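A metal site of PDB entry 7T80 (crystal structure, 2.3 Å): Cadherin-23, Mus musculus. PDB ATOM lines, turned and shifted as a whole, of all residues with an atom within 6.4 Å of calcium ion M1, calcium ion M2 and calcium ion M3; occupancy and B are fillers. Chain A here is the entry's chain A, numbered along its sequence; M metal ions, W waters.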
ATOM      1  N   GLU A  17      10.388  10.131  -5.927  1.00  0.00           N
ATOM      2  CA  GLU A  17       9.203   9.955  -5.046  1.00  0.00           C
ATOM      3  C   GLU A  17       8.060  10.886  -5.459  1.00  0.00           C
ATOM      4  O   GLU A  17       6.959  10.595  -5.030  1.00  0.00           O
ATOM      5  CB  GLU A  17       9.565  10.163  -3.575  1.00  0.00           C
ATOM      6  CG  GLU A  17       9.969  11.576  -3.211  1.00  0.00           C
ATOM      7  CD  GLU A  17       9.994  11.788  -1.710  1.00  0.00           C
ATOM      8  OE1 GLU A  17       9.055  11.240  -1.074  1.00  0.00           O
ATOM      9  OE2 GLU A  17      10.938  12.465  -1.184  1.00  0.00           O
ATOM     10  N   ASN A  18       8.284  11.924  -6.277  1.00  0.00           N
ATOM     11  CA  ASN A  18       7.200  12.826  -6.737  1.00  0.00           C
ATOM     12  C   ASN A  18       6.631  12.394  -8.105  1.00  0.00           C
ATOM     13  O   ASN A  18       5.735  13.118  -8.601  1.00  0.00           O
ATOM     14  CB  ASN A  18       7.647  14.287  -6.791  1.00  0.00           C
ATOM     15  CG  ASN A  18       7.869  14.849  -5.408  1.00  0.00           C
ATOM     16  OD1 ASN A  18       7.622  14.174  -4.409  1.00  0.00           O
ATOM     17  ND2 ASN A  18       8.374  16.061  -5.343  1.00  0.00           N
ATOM     18  N   LEU A  69       3.368   8.361  -4.199  1.00  0.00           N
ATOM     19  CA  LEU A  69       4.505   7.662  -3.569  1.00  0.00           C
ATOM     20  C   LEU A  69       5.108   8.580  -2.506  1.00  0.00           C
ATOM     21  O   LEU A  69       4.871   9.777  -2.593  1.00  0.00           O
ATOM     22  CB  LEU A  69       5.537   7.338  -4.643  1.00  0.00           C
ATOM     23  CG  LEU A  69       5.025   6.546  -5.836  1.00  0.00           C
ATOM     24  CD1 LEU A  69       6.143   6.213  -6.807  1.00  0.00           C
ATOM     25  CD2 LEU A  69       4.358   5.266  -5.392  1.00  0.00           C
ATOM     26  N   ASP A  70       5.876   8.019  -1.574  1.00  0.00           N
ATOM     27  CA  ASP A  70       6.475   8.763  -0.440  1.00  0.00           C
ATOM     28  C   ASP A  70       7.712   7.999   0.037  1.00  0.00           C
ATOM     29  O   ASP A  70       7.542   6.940   0.662  1.00  0.00           O
ATOM     30  CB  ASP A  70       5.446   8.961   0.673  1.00  0.00           C
ATOM     31  CG  ASP A  70       5.927   9.917   1.759  1.00  0.00           C
ATOM     32  OD1 ASP A  70       7.041  10.495   1.599  1.00  0.00           O
ATOM     33  OD2 ASP A  70       5.197  10.087   2.750  1.00  0.00           O
ATOM     34  N   ARG A  71       8.901   8.482  -0.310  1.00  0.00           N
ATOM     35  CA  ARG A  71      10.155   7.802   0.078  1.00  0.00           C
ATOM     36  C   ARG A  71      10.154   7.637   1.600  1.00  0.00           C
ATOM     37  O   ARG A  71      10.681   6.632   2.079  1.00  0.00           O
ATOM     38  CB  ARG A  71      11.372   8.600  -0.362  1.00  0.00           C
ATOM     39  CG  ARG A  71      12.682   7.826  -0.273  1.00  0.00           C
ATOM     40  CD  ARG A  71      13.898   8.746  -0.078  1.00  0.00           C
ATOM     41  NE  ARG A  71      13.740   9.484   1.168  1.00  0.00           N
ATOM     42  CZ  ARG A  71      13.965   8.967   2.370  1.00  0.00           C
ATOM     43  NH1 ARG A  71      14.444   7.735   2.509  1.00  0.00           N
ATOM     44  NH2 ARG A  71      13.770   9.718   3.426  1.00  0.00           N
ATOM     45  N   GLU A  72       9.587   8.622   2.309  1.00  0.00           N
ATOM     46  CA  GLU A  72       9.534   8.700   3.794  1.00  0.00           C
ATOM     47  C   GLU A  72       8.606   7.622   4.356  1.00  0.00           C
ATOM     48  O   GLU A  72       8.713   7.358   5.553  1.00  0.00           O
ATOM     49  CB  GLU A  72       9.062  10.090   4.234  1.00  0.00           C
ATOM     50  CG  GLU A  72      10.164  11.126   4.160  1.00  0.00           C
ATOM     51  CD  GLU A  72      10.618  11.631   2.788  1.00  0.00           C
ATOM     52  OE1 GLU A  72      11.838  11.638   2.569  1.00  0.00           O
ATOM     53  OE2 GLU A  72       9.784  12.134   1.977  1.00  0.00           O
ATOM     54  N   ARG A  73       7.703   7.047   3.535  1.00  0.00           N
ATOM     55  CA  ARG A  73       6.720   6.034   3.990  1.00  0.00           C
ATOM     56  C   ARG A  73       7.187   4.649   3.532  1.00  0.00           C
ATOM     57  O   ARG A  73       7.437   3.806   4.401  1.00  0.00           O
ATOM     58  CB  ARG A  73       5.311   6.349   3.469  1.00  0.00           C
ATOM     59  CG  ARG A  73       4.194   5.963   4.435  1.00  0.00           C
ATOM     60  CD  ARG A  73       2.851   6.556   4.016  1.00  0.00           C
ATOM     61  NE  ARG A  73       2.367   5.736   2.925  1.00  0.00           N
ATOM     62  CZ  ARG A  73       1.745   4.574   3.067  1.00  0.00           C
ATOM     63  NH1 ARG A  73       1.402   3.872   2.003  1.00  0.00           N
ATOM     64  NH2 ARG A  73       1.459   4.100   4.273  1.00  0.00           N
ATOM     65  N   ALA A 105      13.985   7.902  -5.318  1.00  0.00           N
ATOM     66  CA  ALA A 105      14.992   8.964  -5.100  1.00  0.00           C
ATOM     67  C   ALA A 105      14.334  10.042  -4.244  1.00  0.00           C
ATOM     68  O   ALA A 105      13.154  10.366  -4.482  1.00  0.00           O
ATOM     69  CB  ALA A 105      15.449   9.538  -6.411  1.00  0.00           C
ATOM     70  N   ASP A 106      15.092  10.589  -3.305  1.00  0.00           N
ATOM     71  CA  ASP A 106      14.591  11.557  -2.308  1.00  0.00           C
ATOM     72  C   ASP A 106      14.338  12.908  -2.971  1.00  0.00           C
ATOM     73  O   ASP A 106      15.266  13.447  -3.564  1.00  0.00           O
ATOM     74  CB  ASP A 106      15.595  11.746  -1.171  1.00  0.00           C
ATOM     75  CG  ASP A 106      15.002  12.571  -0.027  1.00  0.00           C
ATOM     76  OD1 ASP A 106      13.783  12.408   0.277  1.00  0.00           O
ATOM     77  OD2 ASP A 106      15.757  13.371   0.532  1.00  0.00           O
ATOM     78  N   GLU A 107      13.134  13.446  -2.811  1.00  0.00           N
ATOM     79  CA  GLU A 107      12.814  14.863  -3.115  1.00  0.00           C
ATOM     80  C   GLU A 107      12.780  15.650  -1.793  1.00  0.00           C
ATOM     81  O   GLU A 107      12.486  15.071  -0.701  1.00  0.00           O
ATOM     82  CB  GLU A 107      11.504  14.996  -3.896  1.00  0.00           C
ATOM     83  CG  GLU A 107      11.508  14.365  -5.274  1.00  0.00           C
ATOM     84  CD  GLU A 107      12.526  14.933  -6.248  1.00  0.00           C
ATOM     85  OE1 GLU A 107      12.916  16.094  -6.068  1.00  0.00           O
ATOM     86  OE2 GLU A 107      12.944  14.216  -7.185  1.00  0.00           O
ATOM     87  N   ASN A 108      13.122  16.929  -1.879  1.00  0.00           N
ATOM     88  CA  ASN A 108      13.102  17.852  -0.728  1.00  0.00           C
ATOM     89  C   ASN A 108      11.656  18.256  -0.440  1.00  0.00           C
ATOM     90  O   ASN A 108      11.337  19.370  -0.774  1.00  0.00           O
ATOM     91  CB  ASN A 108      13.963  19.101  -0.998  1.00  0.00           C
ATOM     92  CG  ASN A 108      14.348  19.808   0.272  1.00  0.00           C
ATOM     93  OD1 ASN A 108      14.437  19.188   1.322  1.00  0.00           O
ATOM     94  ND2 ASN A 108      14.599  21.103   0.205  1.00  0.00           N
ATOM     95  N   ASP A 109      10.834  17.372   0.124  1.00  0.00           N
ATOM     96  CA  ASP A 109       9.390  17.655   0.377  1.00  0.00           C
ATOM     97  C   ASP A 109       9.158  17.805   1.890  1.00  0.00           C
ATOM     98  O   ASP A 109       7.992  17.853   2.313  1.00  0.00           O
ATOM     99  CB  ASP A 109       8.453  16.603  -0.254  1.00  0.00           C
ATOM    100  CG  ASP A 109       8.767  15.142   0.039  1.00  0.00           C
ATOM    101  OD1 ASP A 109       9.811  14.888   0.624  1.00  0.00           O
ATOM    102  OD2 ASP A 109       7.947  14.246  -0.356  1.00  0.00           O
ATOM    103  N   ASN A 110      10.205  17.865   2.690  1.00  0.00           N
ATOM    104  CA  ASN A 110      10.069  18.057   4.155  1.00  0.00           C
ATOM    105  C   ASN A 110      10.952  19.216   4.595  1.00  0.00           C
ATOM    106  O   ASN A 110      12.004  19.465   3.963  1.00  0.00           O
ATOM    107  CB  ASN A 110      10.415  16.799   4.957  1.00  0.00           C
ATOM    108  CG  ASN A 110       9.462  15.658   4.671  1.00  0.00           C
ATOM    109  OD1 ASN A 110       8.484  15.472   5.385  1.00  0.00           O
ATOM    110  ND2 ASN A 110       9.761  14.895   3.626  1.00  0.00           N
ATOM    111  N   HIS A 111      10.537  19.915   5.643  1.00  0.00           N
ATOM    112  CA  HIS A 111      11.278  21.068   6.207  1.00  0.00           C
ATOM    113  C   HIS A 111      11.646  20.773   7.645  1.00  0.00           C
ATOM    114  O   HIS A 111      11.023  19.917   8.291  1.00  0.00           O
ATOM    115  CB  HIS A 111      10.501  22.388   6.003  1.00  0.00           C
ATOM    116  CG  HIS A 111       9.186  22.427   6.701  1.00  0.00           C
ATOM    117  ND1 HIS A 111       9.055  22.914   8.010  1.00  0.00           N
ATOM    118  CD2 HIS A 111       7.957  22.058   6.285  1.00  0.00           C
ATOM    119  CE1 HIS A 111       7.789  22.830   8.359  1.00  0.00           C
ATOM    120  NE2 HIS A 111       7.093  22.308   7.324  1.00  0.00           N
ATOM    121  N   PRO A 112      12.705  21.430   8.155  1.00  0.00           N
ATOM    122  CA  PRO A 112      13.103  21.284   9.551  1.00  0.00           C
ATOM    123  C   PRO A 112      11.944  21.672  10.484  1.00  0.00           C
ATOM    124  O   PRO A 112      11.347  22.687  10.275  1.00  0.00           O
ATOM    125  CB  PRO A 112      14.282  22.245   9.693  1.00  0.00           C
ATOM    126  CG  PRO A 112      14.765  22.475   8.269  1.00  0.00           C
ATOM    127  CD  PRO A 112      13.511  22.424   7.432  1.00  0.00           C
ATOM    128  N   ASP A 144      14.676  17.145  10.077  1.00  0.00           N
ATOM    129  CA  ASP A 144      14.145  17.139   8.687  1.00  0.00           C
ATOM    130  C   ASP A 144      14.072  15.672   8.271  1.00  0.00           C
ATOM    131  O   ASP A 144      15.144  15.023   8.223  1.00  0.00           O
ATOM    132  CB  ASP A 144      14.958  18.075   7.796  1.00  0.00           C
ATOM    133  CG  ASP A 144      14.441  18.258   6.369  1.00  0.00           C
ATOM    134  OD1 ASP A 144      14.219  17.231   5.685  1.00  0.00           O
ATOM    135  OD2 ASP A 144      14.355  19.416   5.896  1.00  0.00           O
ATOM    136  N   ALA A 145      12.855  15.207   7.943  1.00  0.00           N
ATOM    137  CA  ALA A 145      12.508  13.820   7.592  1.00  0.00           C
ATOM    138  C   ALA A 145      13.100  13.390   6.236  1.00  0.00           C
ATOM    139  O   ALA A 145      12.934  12.232   5.898  1.00  0.00           O
ATOM    140  CB  ALA A 145      10.999  13.676   7.574  1.00  0.00           C
ATOM    141  N   ASP A 146      13.759  14.246   5.473  1.00  0.00           N
ATOM    142  CA  ASP A 146      14.298  13.821   4.143  1.00  0.00           C
ATOM    143  C   ASP A 146      15.495  12.881   4.389  1.00  0.00           C
ATOM    144  O   ASP A 146      15.778  12.608   5.567  1.00  0.00           O
ATOM    145  CB  ASP A 146      14.571  15.040   3.276  1.00  0.00           C
ATOM    146  CG  ASP A 146      13.298  15.698   2.780  1.00  0.00           C
ATOM    147  OD1 ASP A 146      12.453  14.950   2.206  1.00  0.00           O
ATOM    148  OD2 ASP A 146      13.178  16.951   2.954  1.00  0.00           O
ATOM    149  N   GLU A 147      16.121  12.359   3.341  1.00  0.00           N
ATOM    150  CA  GLU A 147      16.995  11.154   3.421  1.00  0.00           C
ATOM    151  C   GLU A 147      18.367  11.509   4.008  1.00  0.00           C
ATOM    152  O   GLU A 147      18.720  10.903   5.031  1.00  0.00           O
ATOM    153  CB  GLU A 147      17.149  10.482   2.054  1.00  0.00           C
ATOM    154  CG  GLU A 147      18.178   9.349   2.057  1.00  0.00           C
ATOM    155  CD  GLU A 147      18.030   8.381   0.897  1.00  0.00           C
ATOM    156  OE1 GLU A 147      17.800   8.828  -0.247  1.00  0.00           O
ATOM    157  OE2 GLU A 147      18.114   7.168   1.152  1.00  0.00           O
ATOM    158  N   TYR A 150      19.154  16.479   1.810  1.00  0.00           N
ATOM    159  CA  TYR A 150      17.977  17.364   1.941  1.00  0.00           C
ATOM    160  C   TYR A 150      17.515  17.441   3.400  1.00  0.00           C
ATOM    161  O   TYR A 150      16.469  18.007   3.664  1.00  0.00           O
ATOM    162  CB  TYR A 150      16.893  16.854   0.984  1.00  0.00           C
ATOM    163  CG  TYR A 150      17.184  17.086  -0.472  1.00  0.00           C
ATOM    164  CD1 TYR A 150      17.735  18.283  -0.896  1.00  0.00           C
ATOM    165  CD2 TYR A 150      16.848  16.145  -1.433  1.00  0.00           C
ATOM    166  CE1 TYR A 150      17.945  18.543  -2.235  1.00  0.00           C
ATOM    167  CE2 TYR A 150      17.077  16.383  -2.784  1.00  0.00           C
ATOM    168  CZ  TYR A 150      17.636  17.572  -3.180  1.00  0.00           C
ATOM    169  OH  TYR A 150      17.884  17.852  -4.503  1.00  0.00           O
ATOM    170  N   ALA A 151      18.240  16.822   4.328  1.00  0.00           N
ATOM    171  CA  ALA A 151      17.873  16.765   5.756  1.00  0.00           C
ATOM    172  C   ALA A 151      18.941  17.455   6.606  1.00  0.00           C
ATOM    173  O   ALA A 151      18.701  17.589   7.826  1.00  0.00           O
ATOM    174  CB  ALA A 151      17.672  15.320   6.154  1.00  0.00           C
ATOM    175  N   VAL A 152      20.076  17.870   6.029  1.00  0.00           N
ATOM    176  CA  VAL A 152      21.100  18.650   6.777  1.00  0.00           C
ATOM    177  C   VAL A 152      20.487  20.008   7.139  1.00  0.00           C
ATOM    178  O   VAL A 152      20.001  20.721   6.246  1.00  0.00           O
ATOM    179  CB  VAL A 152      22.448  18.801   6.025  1.00  0.00           C
ATOM    180  CG1 VAL A 152      23.388  19.738   6.785  1.00  0.00           C
ATOM    181  CG2 VAL A 152      23.109  17.440   5.810  1.00  0.00           C
ATOM    182  N   ASP A 200      17.123  23.908   5.497  1.00  0.00           N
ATOM    183  CA  ASP A 200      17.756  22.815   4.719  1.00  0.00           C
ATOM    184  C   ASP A 200      18.402  23.474   3.508  1.00  0.00           C
ATOM    185  O   ASP A 200      18.279  24.695   3.375  1.00  0.00           O
ATOM    186  CB  ASP A 200      16.769  21.686   4.456  1.00  0.00           C
ATOM    187  CG  ASP A 200      15.713  21.943   3.403  1.00  0.00           C
ATOM    188  OD1 ASP A 200      15.825  22.967   2.666  1.00  0.00           O
ATOM    189  OD2 ASP A 200      14.783  21.112   3.303  1.00  0.00           O
ATOM    190  N   ILE A 201      19.076  22.703   2.658  1.00  0.00           N
ATOM    191  CA  ILE A 201      19.910  23.236   1.542  1.00  0.00           C
ATOM    192  C   ILE A 201      19.013  23.676   0.388  1.00  0.00           C
ATOM    193  O   ILE A 201      19.516  24.352  -0.521  1.00  0.00           O
ATOM    194  CB  ILE A 201      20.973  22.177   1.138  1.00  0.00           C
ATOM    195  CG1 ILE A 201      22.175  22.831   0.437  1.00  0.00           C
ATOM    196  CG2 ILE A 201      20.358  21.040   0.318  1.00  0.00           C
ATOM    197  CD1 ILE A 201      23.061  23.673   1.368  1.00  0.00           C
ATOM    198  N   LEU A 204      14.154  25.471   2.479  1.00  0.00           N
ATOM    199  CA  LEU A 204      12.898  25.211   3.249  1.00  0.00           C
ATOM    200  C   LEU A 204      13.235  25.405   4.734  1.00  0.00           C
ATOM    201  O   LEU A 204      14.200  24.844   5.192  1.00  0.00           O
ATOM    202  CB  LEU A 204      12.362  23.804   2.956  1.00  0.00           C
ATOM    203  CG  LEU A 204      12.007  23.455   1.509  1.00  0.00           C
ATOM    204  CD1 LEU A 204      11.167  22.187   1.457  1.00  0.00           C
ATOM    205  CD2 LEU A 204      11.264  24.578   0.811  1.00  0.00           C
HETATM  206 CA    CA M   1      11.700  13.370   0.755  1.00  0.00          CA
HETATM  207 CA    CA M   2      14.305  18.865   3.653  1.00  0.00          CA
HETATM  208 CA    CA M   3       7.890  12.432   0.652  1.00  0.00          CA
HETATM  209  O   HOH W   1       5.826  12.420  -0.486  1.00  0.00           O
HETATM  210  O   HOH W   2       7.079  13.677   2.541  1.00  0.00           O
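The nearest printed residue that does not touch calcium ion M1 is Arg 71 (4.4 Å).
Four residues have an atom within 4 Å of calcium ion M3: Glu 17, Asp 70, Glu 72 and Asp 109.
The nearest printed residue that does not touch calcium ion M3 is Arg 71 (4.2 Å).
Calcium ion M2 is bound by OD2 of Asp 144 (2.3 Å), OD2 of Asp 200 (2.3 Å), O of Tyr 150 (2.3 Å), OD2 of Asp 146 (2.3 Å), OD1 of Asn 108 (2.4 Å), O of Asn 110 (2.4 Å) and OD1 of Asp 144 (2.6 Å).
Calcium ion M2 has seven donor atoms within binding distance.
Within 4 Å of calcium ion M2: Asn 108, Asn 110, Asp 144, Asp 146, Tyr 150 and Asp 200.
Along chain A the residues within 4 Å of calcium ion M2 span positions 108 to 200.
The nearest printed residue that does not touch calcium ion M2 is His 111 (4.4 Å).
The side-chain carboxylate (OD2) of Asp 109 is bound to calcium ion M3 (2.1 Å).
The side-chain carboxylate (OD1) of Asp 70 is bound to calcium ion M3, 2.3 Å away.
The side-chain carboxylate (OE2) of Glu 72 is bound to calcium ion M3.
Calcium ion M3 is bound by water W1, at 2.4 Å.
Calcium ion M3 is bound by OE1 of Glu 17 (2.4 Å).
Calcium ion M3 is bound by water W2 (2.4 Å).
Slightly farther from calcium ion M3 lies the side-chain carboxylate (OD1) of Asp 109 (3.1 Å).
Calcium ion M1 is bound by OE2 of Glu 17 (2.3 Å), OD1 of Asp 146 (2.3 Å), OD1 of Asp 106 (2.3 Å), O of Glu 107 (2.4 Å), OD1 of Asp 109 (2.4 Å), OE1 of Glu 72 (2.5 Å) and OE2 of Glu 72 (2.6 Å).
N of Glu 17 sits at hydrogen-bond distance from O of Ala 105, at 3.1 Å.
The backbone NH (N) of Leu 204 sits at hydrogen-bond distance from the side-chain carboxylate (OD1) of Asp 200, at 3.0 Å.
The side-chain carboxylate (OE1) of Glu 72 sits close to the guanidinium group (NH2) of Arg 71 (2.9 Å).
OD2 of Asp 106 lies within hydrogen-bond range of N of Glu 147, 3.0 Å away.
The side-chain carboxylate (OD1) of Asp 106 sits close to the guanidinium group (NE) of Arg 71 (3.1 Å).
The backbone NH of Arg 71 sits close to the side-chain carboxylate of Glu 17 (2.9 Å).
The side-chain carboxylate of Asp 109 sits close to the side-chain amide nitrogen of Asn 110 (3.0 Å).
The side-chain amide nitrogen (ND2) of Asn 110 lies close to the side-chain carboxylate (OE2) of Glu 72 (3.2 Å).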
